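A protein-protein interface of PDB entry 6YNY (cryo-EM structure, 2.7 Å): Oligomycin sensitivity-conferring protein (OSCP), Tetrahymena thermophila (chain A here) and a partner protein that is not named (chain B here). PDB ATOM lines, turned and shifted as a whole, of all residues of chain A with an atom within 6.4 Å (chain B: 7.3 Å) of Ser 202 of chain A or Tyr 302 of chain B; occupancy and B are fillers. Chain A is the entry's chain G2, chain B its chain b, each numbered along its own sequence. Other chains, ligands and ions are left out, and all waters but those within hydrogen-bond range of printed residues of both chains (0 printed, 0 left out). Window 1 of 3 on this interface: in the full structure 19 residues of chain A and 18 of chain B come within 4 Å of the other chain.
O of Gly 188 of chain A touches CB of Ser 287 of chain B, 3.7 Å away.
Leu 190 of chain A touches Ala 291 of chain B.
Met 300 of chain B touches Asp 200 of chain A.
OH of Tyr 302 of chain B touches O of Asp 200 of chain A (3.9 Å).
SG of Cys 201 of chain A touches CG of Met 300 of chain B, at 3.9 Å.
Cys 201 of chain A touches Tyr 302 of chain B.
Leu 203 of chain A touches Ser 287 of chain B (CD1 to OG, 3.0 Å).
Leu 203 of chain A touches Leu 307 of chain B.
NH1 of Arg 206 of chain A touches CD2 of Leu 308 of chain B, at 3.7 Å.
CG2 of Val 207 of chain A touches CD1 of Leu 307 of chain B, at 3.5 Å.
Of the 14 printed residues of chain B, 7 touch a printed residue of chain A.
Of the 15 printed residues of chain A, 9 touch a printed residue of chain B.
Printed residues of chain A that touch a printed residue of chain B: Gly 188, Leu 190, Leu 199, Asp 200, Cys 201, Ser 202, Leu 203, Arg 206 and Val 207.
Hydrophobic or aromatic side chains of chain A within 4 Å of the printed part of chain B: Leu 190, Leu 199, Leu 203 and Val 207.
Among the printed residues, 16 pairs touch across the chains.
Among the printed residues, Asp or Glu carboxylates within 4 Å of a Lys or Arg side-chain nitrogen of the other chain: Arg 206 of chain A with Asp 305 of chain B.
The side-chain carboxylate (OD1) of Asp 200 of chain A sits at hydrogen-bond distance from the side-chain hydroxyl (OG) of Ser 202 of chain A (2.6 Å).
The side-chain carboxylate of Asp 305 of chain B sits close to the backbone carbonyl oxygen of Tyr 302 of chain B (2.7 Å).
OD2 of Asp 200 of chain A lies close to OG of Ser 205 of chain A, 3.4 Å away.
N of Ser 202 of chain A is in hydrogen-bond range of O of Leu 190 of chain A, 3.1 Å away.
The side-chain amide oxygen (OE1) of Gln 191 of chain A sits close to the side-chain carboxylate (OD1) of Asp 200 of chain A, 3.3 Å away.
The backbone NH (N) of Cys 201 of chain A is in hydrogen-bond range of the backbone carbonyl oxygen (O) of Leu 190 of chain A, 2.9 Å away.
Printed residues of chain B within 4 Å of Gly 188 of chain A: Ser 287 (3.7 Å).
Of the printed residues of chain B, Leu 199 of chain A touches Met 300 (3.8 Å).
Ser 202 of chain A touches just one residue of chain B: Tyr 302 (2.9 Å).
Of the printed residues of chain B, Leu 203 of chain A touches Ser 287 (3.0 Å) and Leu 307 (3.8 Å).
Asp 301 of chain B touches none of the printed residues of chain A.
Printed residues of chain A within 4 Å of Tyr 302 of chain B: Asp 200 (3.9 Å), Cys 201 (3.6 Å), Ser 202 (2.9 Å) and Arg 206 (3.6 Å).
Pro 309 of chain B touches none of the printed residues of chain A.
The backbone carbonyl oxygen of Ala 291 of chain B sits at hydrogen-bond distance from the side-chain sulfur of Cys 201 of chain A.
The backbone carbonyl oxygen (O) of Ser 202 of chain A sits at hydrogen-bond distance from the side-chain hydroxyl (OH) of Tyr 302 of chain B, 2.9 Å away.
The guanidinium group of Arg 206 of chain A is in salt-bridge range of the side-chain carboxylate of Asp 305 of chain B (2.5 Å).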
ATOM      1  N   ILE A 186      32.698  -2.299  -9.325  1.00  0.00           N
ATOM      2  CA  ILE A 186      31.435  -3.028  -9.368  1.00  0.00           C
ATOM      3  C   ILE A 186      30.490  -2.339 -10.342  1.00  0.00           C
ATOM      4  O   ILE A 186      30.744  -1.212 -10.780  1.00  0.00           O
ATOM      5  CB  ILE A 186      30.804  -3.133  -7.967  1.00  0.00           C
ATOM      6  CG1 ILE A 186      30.487  -1.739  -7.414  1.00  0.00           C
ATOM      7  CG2 ILE A 186      31.732  -3.881  -7.025  1.00  0.00           C
ATOM      8  CD1 ILE A 186      29.936  -1.744  -6.004  1.00  0.00           C
ATOM      9  N   LEU A 187      29.396  -3.014 -10.689  1.00  0.00           N
ATOM     10  CA  LEU A 187      28.377  -2.477 -11.579  1.00  0.00           C
ATOM     11  C   LEU A 187      27.030  -2.517 -10.874  1.00  0.00           C
ATOM     12  O   LEU A 187      26.610  -3.574 -10.390  1.00  0.00           O
ATOM     13  CB  LEU A 187      28.310  -3.268 -12.889  1.00  0.00           C
ATOM     14  CG  LEU A 187      29.549  -3.220 -13.789  1.00  0.00           C
ATOM     15  CD1 LEU A 187      30.635  -4.167 -13.292  1.00  0.00           C
ATOM     16  CD2 LEU A 187      29.174  -3.544 -15.227  1.00  0.00           C
ATOM     17  N   GLY A 188      26.359  -1.369 -10.817  1.00  0.00           N
ATOM     18  CA  GLY A 188      25.045  -1.307 -10.198  1.00  0.00           C
ATOM     19  C   GLY A 188      25.032  -1.745  -8.752  1.00  0.00           C
ATOM     20  O   GLY A 188      24.012  -2.250  -8.271  1.00  0.00           O
ATOM     21  N   GLY A 189      26.142  -1.564  -8.042  1.00  0.00           N
ATOM     22  CA  GLY A 189      26.264  -1.972  -6.655  1.00  0.00           C
ATOM     23  C   GLY A 189      26.351  -0.771  -5.734  1.00  0.00           C
ATOM     24  O   GLY A 189      26.797   0.306  -6.136  1.00  0.00           O
ATOM     25  N   LEU A 190      25.920  -0.962  -4.489  1.00  0.00           N
ATOM     26  CA  LEU A 190      25.923   0.085  -3.475  1.00  0.00           C
ATOM     27  C   LEU A 190      26.811  -0.344  -2.318  1.00  0.00           C
ATOM     28  O   LEU A 190      26.679  -1.461  -1.808  1.00  0.00           O
ATOM     29  CB  LEU A 190      24.506   0.372  -2.968  1.00  0.00           C
ATOM     30  CG  LEU A 190      23.585   1.206  -3.863  1.00  0.00           C
ATOM     31  CD1 LEU A 190      24.141   2.609  -4.056  1.00  0.00           C
ATOM     32  CD2 LEU A 190      23.363   0.527  -5.206  1.00  0.00           C
ATOM     33  N   GLN A 191      27.712   0.547  -1.909  1.00  0.00           N
ATOM     34  CA  GLN A 191      28.598   0.307  -0.774  1.00  0.00           C
ATOM     35  C   GLN A 191      28.674   1.578   0.054  1.00  0.00           C
ATOM     36  O   GLN A 191      29.075   2.628  -0.459  1.00  0.00           O
ATOM     37  CB  GLN A 191      29.994  -0.116  -1.241  1.00  0.00           C
ATOM     38  CG  GLN A 191      30.015  -1.430  -2.012  1.00  0.00           C
ATOM     39  CD  GLN A 191      31.404  -1.830  -2.494  1.00  0.00           C
ATOM     40  OE1 GLN A 191      31.552  -2.818  -3.215  1.00  0.00           O
ATOM     41  NE2 GLN A 191      32.426  -1.072  -2.102  1.00  0.00           N
ATOM     42  N   LEU A 199      28.821  -1.576   5.036  1.00  0.00           N
ATOM     43  CA  LEU A 199      27.729  -2.476   4.685  1.00  0.00           C
ATOM     44  C   LEU A 199      27.705  -2.607   3.171  1.00  0.00           C
ATOM     45  O   LEU A 199      27.597  -1.602   2.462  1.00  0.00           O
ATOM     46  CB  LEU A 199      26.389  -1.952   5.211  1.00  0.00           C
ATOM     47  CG  LEU A 199      25.207  -2.927   5.271  1.00  0.00           C
ATOM     48  CD1 LEU A 199      24.792  -3.385   3.881  1.00  0.00           C
ATOM     49  CD2 LEU A 199      25.531  -4.123   6.155  1.00  0.00           C
ATOM     50  N   ASP A 200      27.804  -3.840   2.680  1.00  0.00           N
ATOM     51  CA  ASP A 200      27.907  -4.113   1.250  1.00  0.00           C
ATOM     52  C   ASP A 200      26.540  -4.520   0.712  1.00  0.00           C
ATOM     53  O   ASP A 200      26.006  -5.571   1.081  1.00  0.00           O
ATOM     54  CB  ASP A 200      28.941  -5.205   0.983  1.00  0.00           C
ATOM     55  CG  ASP A 200      29.074  -5.531  -0.490  1.00  0.00           C
ATOM     56  OD1 ASP A 200      29.596  -4.684  -1.244  1.00  0.00           O
ATOM     57  OD2 ASP A 200      28.654  -6.637  -0.896  1.00  0.00           O
ATOM     58  N   CYS A 201      25.979  -3.683  -0.160  1.00  0.00           N
ATOM     59  CA  CYS A 201      24.769  -4.002  -0.908  1.00  0.00           C
ATOM     60  C   CYS A 201      25.057  -4.180  -2.394  1.00  0.00           C
ATOM     61  O   CYS A 201      24.135  -4.129  -3.214  1.00  0.00           O
ATOM     62  CB  CYS A 201      23.714  -2.914  -0.704  1.00  0.00           C
ATOM     63  SG  CYS A 201      23.205  -2.674   1.012  1.00  0.00           S
ATOM     64  N   SER A 202      26.321  -4.387  -2.754  1.00  0.00           N
ATOM     65  CA  SER A 202      26.708  -4.425  -4.155  1.00  0.00           C
ATOM     66  C   SER A 202      26.210  -5.699  -4.826  1.00  0.00           C
ATOM     67  O   SER A 202      26.206  -6.778  -4.228  1.00  0.00           O
ATOM     68  CB  SER A 202      28.226  -4.328  -4.286  1.00  0.00           C
ATOM     69  OG  SER A 202      28.866  -5.382  -3.589  1.00  0.00           O
ATOM     70  N   LEU A 203      25.786  -5.562  -6.084  1.00  0.00           N
ATOM     71  CA  LEU A 203      25.411  -6.732  -6.871  1.00  0.00           C
ATOM     72  C   LEU A 203      26.616  -7.611  -7.175  1.00  0.00           C
ATOM     73  O   LEU A 203      26.464  -8.824  -7.357  1.00  0.00           O
ATOM     74  CB  LEU A 203      24.732  -6.292  -8.168  1.00  0.00           C
ATOM     75  CG  LEU A 203      24.407  -7.402  -9.174  1.00  0.00           C
ATOM     76  CD1 LEU A 203      23.085  -7.118  -9.864  1.00  0.00           C
ATOM     77  CD2 LEU A 203      25.519  -7.554 -10.205  1.00  0.00           C
ATOM     78  N   LEU A 204      27.813  -7.024  -7.235  1.00  0.00           N
ATOM     79  CA  LEU A 204      29.009  -7.817  -7.500  1.00  0.00           C
ATOM     80  C   LEU A 204      29.189  -8.901  -6.446  1.00  0.00           C
ATOM     81  O   LEU A 204      29.582 -10.029  -6.764  1.00  0.00           O
ATOM     82  CB  LEU A 204      30.235  -6.901  -7.558  1.00  0.00           C
ATOM     83  CG  LEU A 204      31.604  -7.523  -7.859  1.00  0.00           C
ATOM     84  CD1 LEU A 204      32.239  -8.122  -6.608  1.00  0.00           C
ATOM     85  CD2 LEU A 204      31.500  -8.571  -8.960  1.00  0.00           C
ATOM     86  N   SER A 205      28.903  -8.581  -5.181  1.00  0.00           N
ATOM     87  CA  SER A 205      28.999  -9.588  -4.130  1.00  0.00           C
ATOM     88  C   SER A 205      28.012 -10.721  -4.372  1.00  0.00           C
ATOM     89  O   SER A 205      28.327 -11.893  -4.128  1.00  0.00           O
ATOM     90  CB  SER A 205      28.752  -8.944  -2.766  1.00  0.00           C
ATOM     91  OG  SER A 205      28.817  -9.907  -1.728  1.00  0.00           O
ATOM     92  N   ARG A 206      26.811 -10.393  -4.851  1.00  0.00           N
ATOM     93  CA  ARG A 206      25.819 -11.423  -5.139  1.00  0.00           C
ATOM     94  C   ARG A 206      26.294 -12.349  -6.251  1.00  0.00           C
ATOM     95  O   ARG A 206      26.133 -13.572  -6.162  1.00  0.00           O
ATOM     96  CB  ARG A 206      24.487 -10.770  -5.515  1.00  0.00           C
ATOM     97  CG  ARG A 206      23.352 -11.751  -5.770  1.00  0.00           C
ATOM     98  CD  ARG A 206      23.028 -12.570  -4.532  1.00  0.00           C
ATOM     99  NE  ARG A 206      21.817 -13.369  -4.703  1.00  0.00           N
ATOM    100  CZ  ARG A 206      21.279 -14.127  -3.752  1.00  0.00           C
ATOM    101  NH1 ARG A 206      20.175 -14.819  -4.001  1.00  0.00           N
ATOM    102  NH2 ARG A 206      21.842 -14.198  -2.553  1.00  0.00           N
ATOM    103  N   VAL A 207      26.887 -11.787  -7.305  1.00  0.00           N
ATOM    104  CA  VAL A 207      27.326 -12.601  -8.436  1.00  0.00           C
ATOM    105  C   VAL A 207      28.361 -13.624  -7.983  1.00  0.00           C
ATOM    106  O   VAL A 207      28.251 -14.820  -8.281  1.00  0.00           O
ATOM    107  CB  VAL A 207      27.875 -11.705  -9.560  1.00  0.00           C
ATOM    108  CG1 VAL A 207      28.455 -12.552 -10.682  1.00  0.00           C
ATOM    109  CG2 VAL A 207      26.782 -10.789 -10.091  1.00  0.00           C
ATOM    110  N   SER B 287      18.330  -4.020  -8.653  1.00  0.00           N
ATOM    111  CA  SER B 287      19.437  -4.023  -7.704  1.00  0.00           C
ATOM    112  C   SER B 287      19.407  -2.780  -6.823  1.00  0.00           C
ATOM    113  O   SER B 287      19.665  -2.858  -5.617  1.00  0.00           O
ATOM    114  CB  SER B 287      20.766  -4.115  -8.452  1.00  0.00           C
ATOM    115  OG  SER B 287      20.818  -5.285  -9.249  1.00  0.00           O
ATOM    116  N   SER B 290      16.633  -3.278  -4.229  1.00  0.00           N
ATOM    117  CA  SER B 290      17.097  -4.205  -3.205  1.00  0.00           C
ATOM    118  C   SER B 290      18.239  -3.613  -2.390  1.00  0.00           C
ATOM    119  O   SER B 290      18.438  -3.999  -1.231  1.00  0.00           O
ATOM    120  CB  SER B 290      17.531  -5.522  -3.849  1.00  0.00           C
ATOM    121  OG  SER B 290      17.986  -6.442  -2.872  1.00  0.00           O
ATOM    122  N   ALA B 291      18.998  -2.682  -2.971  1.00  0.00           N
ATOM    123  CA  ALA B 291      20.100  -2.064  -2.240  1.00  0.00           C
ATOM    124  C   ALA B 291      19.581  -1.156  -1.132  1.00  0.00           C
ATOM    125  O   ALA B 291      19.969  -1.297   0.033  1.00  0.00           O
ATOM    126  CB  ALA B 291      20.992  -1.281  -3.204  1.00  0.00           C
ATOM    127  N   ASP B 293      16.826  -1.207   0.301  1.00  0.00           N
ATOM    128  CA  ASP B 293      16.183  -2.027   1.323  1.00  0.00           C
ATOM    129  C   ASP B 293      17.194  -2.479   2.369  1.00  0.00           C
ATOM    130  O   ASP B 293      16.934  -2.405   3.576  1.00  0.00           O
ATOM    131  CB  ASP B 293      15.503  -3.233   0.673  1.00  0.00           C
ATOM    132  CG  ASP B 293      14.832  -4.139   1.686  1.00  0.00           C
ATOM    133  OD1 ASP B 293      13.812  -3.724   2.274  1.00  0.00           O
ATOM    134  OD2 ASP B 293      15.325  -5.267   1.895  1.00  0.00           O
ATOM    135  N   MET B 300      21.677  -6.894   5.113  1.00  0.00           N
ATOM    136  CA  MET B 300      21.343  -6.885   3.694  1.00  0.00           C
ATOM    137  C   MET B 300      21.093  -8.311   3.234  1.00  0.00           C
ATOM    138  O   MET B 300      21.968  -9.173   3.376  1.00  0.00           O
ATOM    139  CB  MET B 300      22.465  -6.243   2.869  1.00  0.00           C
ATOM    140  CG  MET B 300      22.330  -6.448   1.366  1.00  0.00           C
ATOM    141  SD  MET B 300      20.723  -5.937   0.729  1.00  0.00           S
ATOM    142  CE  MET B 300      20.906  -6.344  -1.004  1.00  0.00           C
ATOM    143  N   ASP B 301      19.906  -8.556   2.684  1.00  0.00           N
ATOM    144  CA  ASP B 301      19.541  -9.850   2.131  1.00  0.00           C
ATOM    145  C   ASP B 301      19.002  -9.651   0.723  1.00  0.00           C
ATOM    146  O   ASP B 301      18.254  -8.704   0.462  1.00  0.00           O
ATOM    147  CB  ASP B 301      18.499 -10.557   3.002  1.00  0.00           C
ATOM    148  CG  ASP B 301      19.063 -11.020   4.330  1.00  0.00           C
ATOM    149  OD1 ASP B 301      20.259 -10.772   4.589  1.00  0.00           O
ATOM    150  OD2 ASP B 301      18.312 -11.637   5.113  1.00  0.00           O
ATOM    151  N   TYR B 302      19.388 -10.548  -0.182  1.00  0.00           N
ATOM    152  CA  TYR B 302      19.012 -10.448  -1.592  1.00  0.00           C
ATOM    153  C   TYR B 302      17.745 -11.255  -1.887  1.00  0.00           C
ATOM    154  O   TYR B 302      17.746 -12.208  -2.665  1.00  0.00           O
ATOM    155  CB  TYR B 302      20.172 -10.900  -2.472  1.00  0.00           C
ATOM    156  CG  TYR B 302      21.418 -10.057  -2.323  1.00  0.00           C
ATOM    157  CD1 TYR B 302      21.682  -9.013  -3.200  1.00  0.00           C
ATOM    158  CD2 TYR B 302      22.329 -10.303  -1.305  1.00  0.00           C
ATOM    159  CE1 TYR B 302      22.819  -8.240  -3.067  1.00  0.00           C
ATOM    160  CE2 TYR B 302      23.469  -9.534  -1.164  1.00  0.00           C
ATOM    161  CZ  TYR B 302      23.709  -8.504  -2.048  1.00  0.00           C
ATOM    162  OH  TYR B 302      24.842  -7.736  -1.912  1.00  0.00           O
ATOM    163  N   GLN B 303      16.644 -10.858  -1.244  1.00  0.00           N
ATOM    164  CA  GLN B 303      15.374 -11.529  -1.504  1.00  0.00           C
ATOM    165  C   GLN B 303      14.761 -11.091  -2.827  1.00  0.00           C
ATOM    166  O   GLN B 303      14.019 -11.862  -3.445  1.00  0.00           O
ATOM    167  CB  GLN B 303      14.377 -11.264  -0.373  1.00  0.00           C
ATOM    168  CG  GLN B 303      14.763 -11.856   0.971  1.00  0.00           C
ATOM    169  CD  GLN B 303      15.507 -10.876   1.850  1.00  0.00           C
ATOM    170  OE1 GLN B 303      16.094  -9.908   1.367  1.00  0.00           O
ATOM    171  NE2 GLN B 303      15.477 -11.115   3.156  1.00  0.00           N
ATOM    172  N   ASN B 304      15.057  -9.871  -3.276  1.00  0.00           N
ATOM    173  CA  ASN B 304      14.467  -9.311  -4.484  1.00  0.00           C
ATOM    174  C   ASN B 304      15.469  -9.202  -5.627  1.00  0.00           C
ATOM    175  O   ASN B 304      15.192  -8.516  -6.617  1.00  0.00           O
ATOM    176  CB  ASN B 304      13.867  -7.936  -4.185  1.00  0.00           C
ATOM    177  CG  ASN B 304      12.819  -7.984  -3.091  1.00  0.00           C
ATOM    178  OD1 ASN B 304      12.107  -8.976  -2.940  1.00  0.00           O
ATOM    179  ND2 ASN B 304      12.720  -6.907  -2.320  1.00  0.00           N
ATOM    180  N   ASP B 305      16.620  -9.856  -5.519  1.00  0.00           N
ATOM    181  CA  ASP B 305      17.614  -9.774  -6.577  1.00  0.00           C
ATOM    182  C   ASP B 305      17.119 -10.511  -7.819  1.00  0.00           C
ATOM    183  O   ASP B 305      16.537 -11.595  -7.708  1.00  0.00           O
ATOM    184  CB  ASP B 305      18.942 -10.369  -6.112  1.00  0.00           C
ATOM    185  CG  ASP B 305      18.832 -11.840  -5.765  1.00  0.00           C
ATOM    186  OD1 ASP B 305      17.741 -12.269  -5.334  1.00  0.00           O
ATOM    187  OD2 ASP B 305      19.834 -12.567  -5.925  1.00  0.00           O
ATOM    188  N   PRO B 306      17.333  -9.955  -9.018  1.00  0.00           N
ATOM    189  CA  PRO B 306      16.871 -10.634 -10.235  1.00  0.00           C
ATOM    190  C   PRO B 306      17.817 -11.713 -10.737  1.00  0.00           C
ATOM    191  O   PRO B 306      17.428 -12.488 -11.622  1.00  0.00           O
ATOM    192  CB  PRO B 306      16.767  -9.487 -11.247  1.00  0.00           C
ATOM    193  CG  PRO B 306      17.830  -8.534 -10.820  1.00  0.00           C
ATOM    194  CD  PRO B 306      17.937  -8.644  -9.317  1.00  0.00           C
ATOM    195  N   LEU B 307      19.038 -11.788 -10.205  1.00  0.00           N
ATOM    196  CA  LEU B 307      19.992 -12.788 -10.674  1.00  0.00           C
ATOM    197  C   LEU B 307      19.514 -14.198 -10.353  1.00  0.00           C
ATOM    198  O   LEU B 307      19.564 -15.092 -11.206  1.00  0.00           O
ATOM    199  CB  LEU B 307      21.365 -12.531 -10.052  1.00  0.00           C
ATOM    200  CG  LEU B 307      21.965 -11.147 -10.311  1.00  0.00           C
ATOM    201  CD1 LEU B 307      23.294 -11.002  -9.587  1.00  0.00           C
ATOM    202  CD2 LEU B 307      22.134 -10.899 -11.803  1.00  0.00           C
ATOM    203  N   LEU B 308      19.044 -14.420  -9.122  1.00  0.00           N
ATOM    204  CA  LEU B 308      18.606 -15.758  -8.728  1.00  0.00           C
ATOM    205  C   LEU B 308      17.457 -16.259  -9.592  1.00  0.00           C
ATOM    206  O   LEU B 308      17.579 -17.346 -10.182  1.00  0.00           O
ATOM    207  CB  LEU B 308      18.240 -15.754  -7.241  1.00  0.00           C
ATOM    208  CG  LEU B 308      17.730 -17.081  -6.673  1.00  0.00           C
ATOM    209  CD1 LEU B 308      18.765 -18.182  -6.850  1.00  0.00           C
ATOM    210  CD2 LEU B 308      17.359 -16.923  -5.207  1.00  0.00           C
ATOM    211  N   PRO B 309      16.335 -15.545  -9.718  1.00  0.00           N
ATOM    212  CA  PRO B 309      15.256 -16.053 -10.580  1.00  0.00           C
ATOM    213  C   PRO B 309      15.681 -16.221 -12.027  1.00  0.00           C
ATOM    214  O   PRO B 309      15.178 -17.120 -12.712  1.00  0.00           O
ATOM    215  CB  PRO B 309      14.154 -14.995 -10.427  1.00  0.00           C
ATOM    216  CG  PRO B 309      14.857 -13.768  -9.956  1.00  0.00           C
ATOM    217  CD  PRO B 309      15.982 -14.254  -9.103  1.00  0.00           C
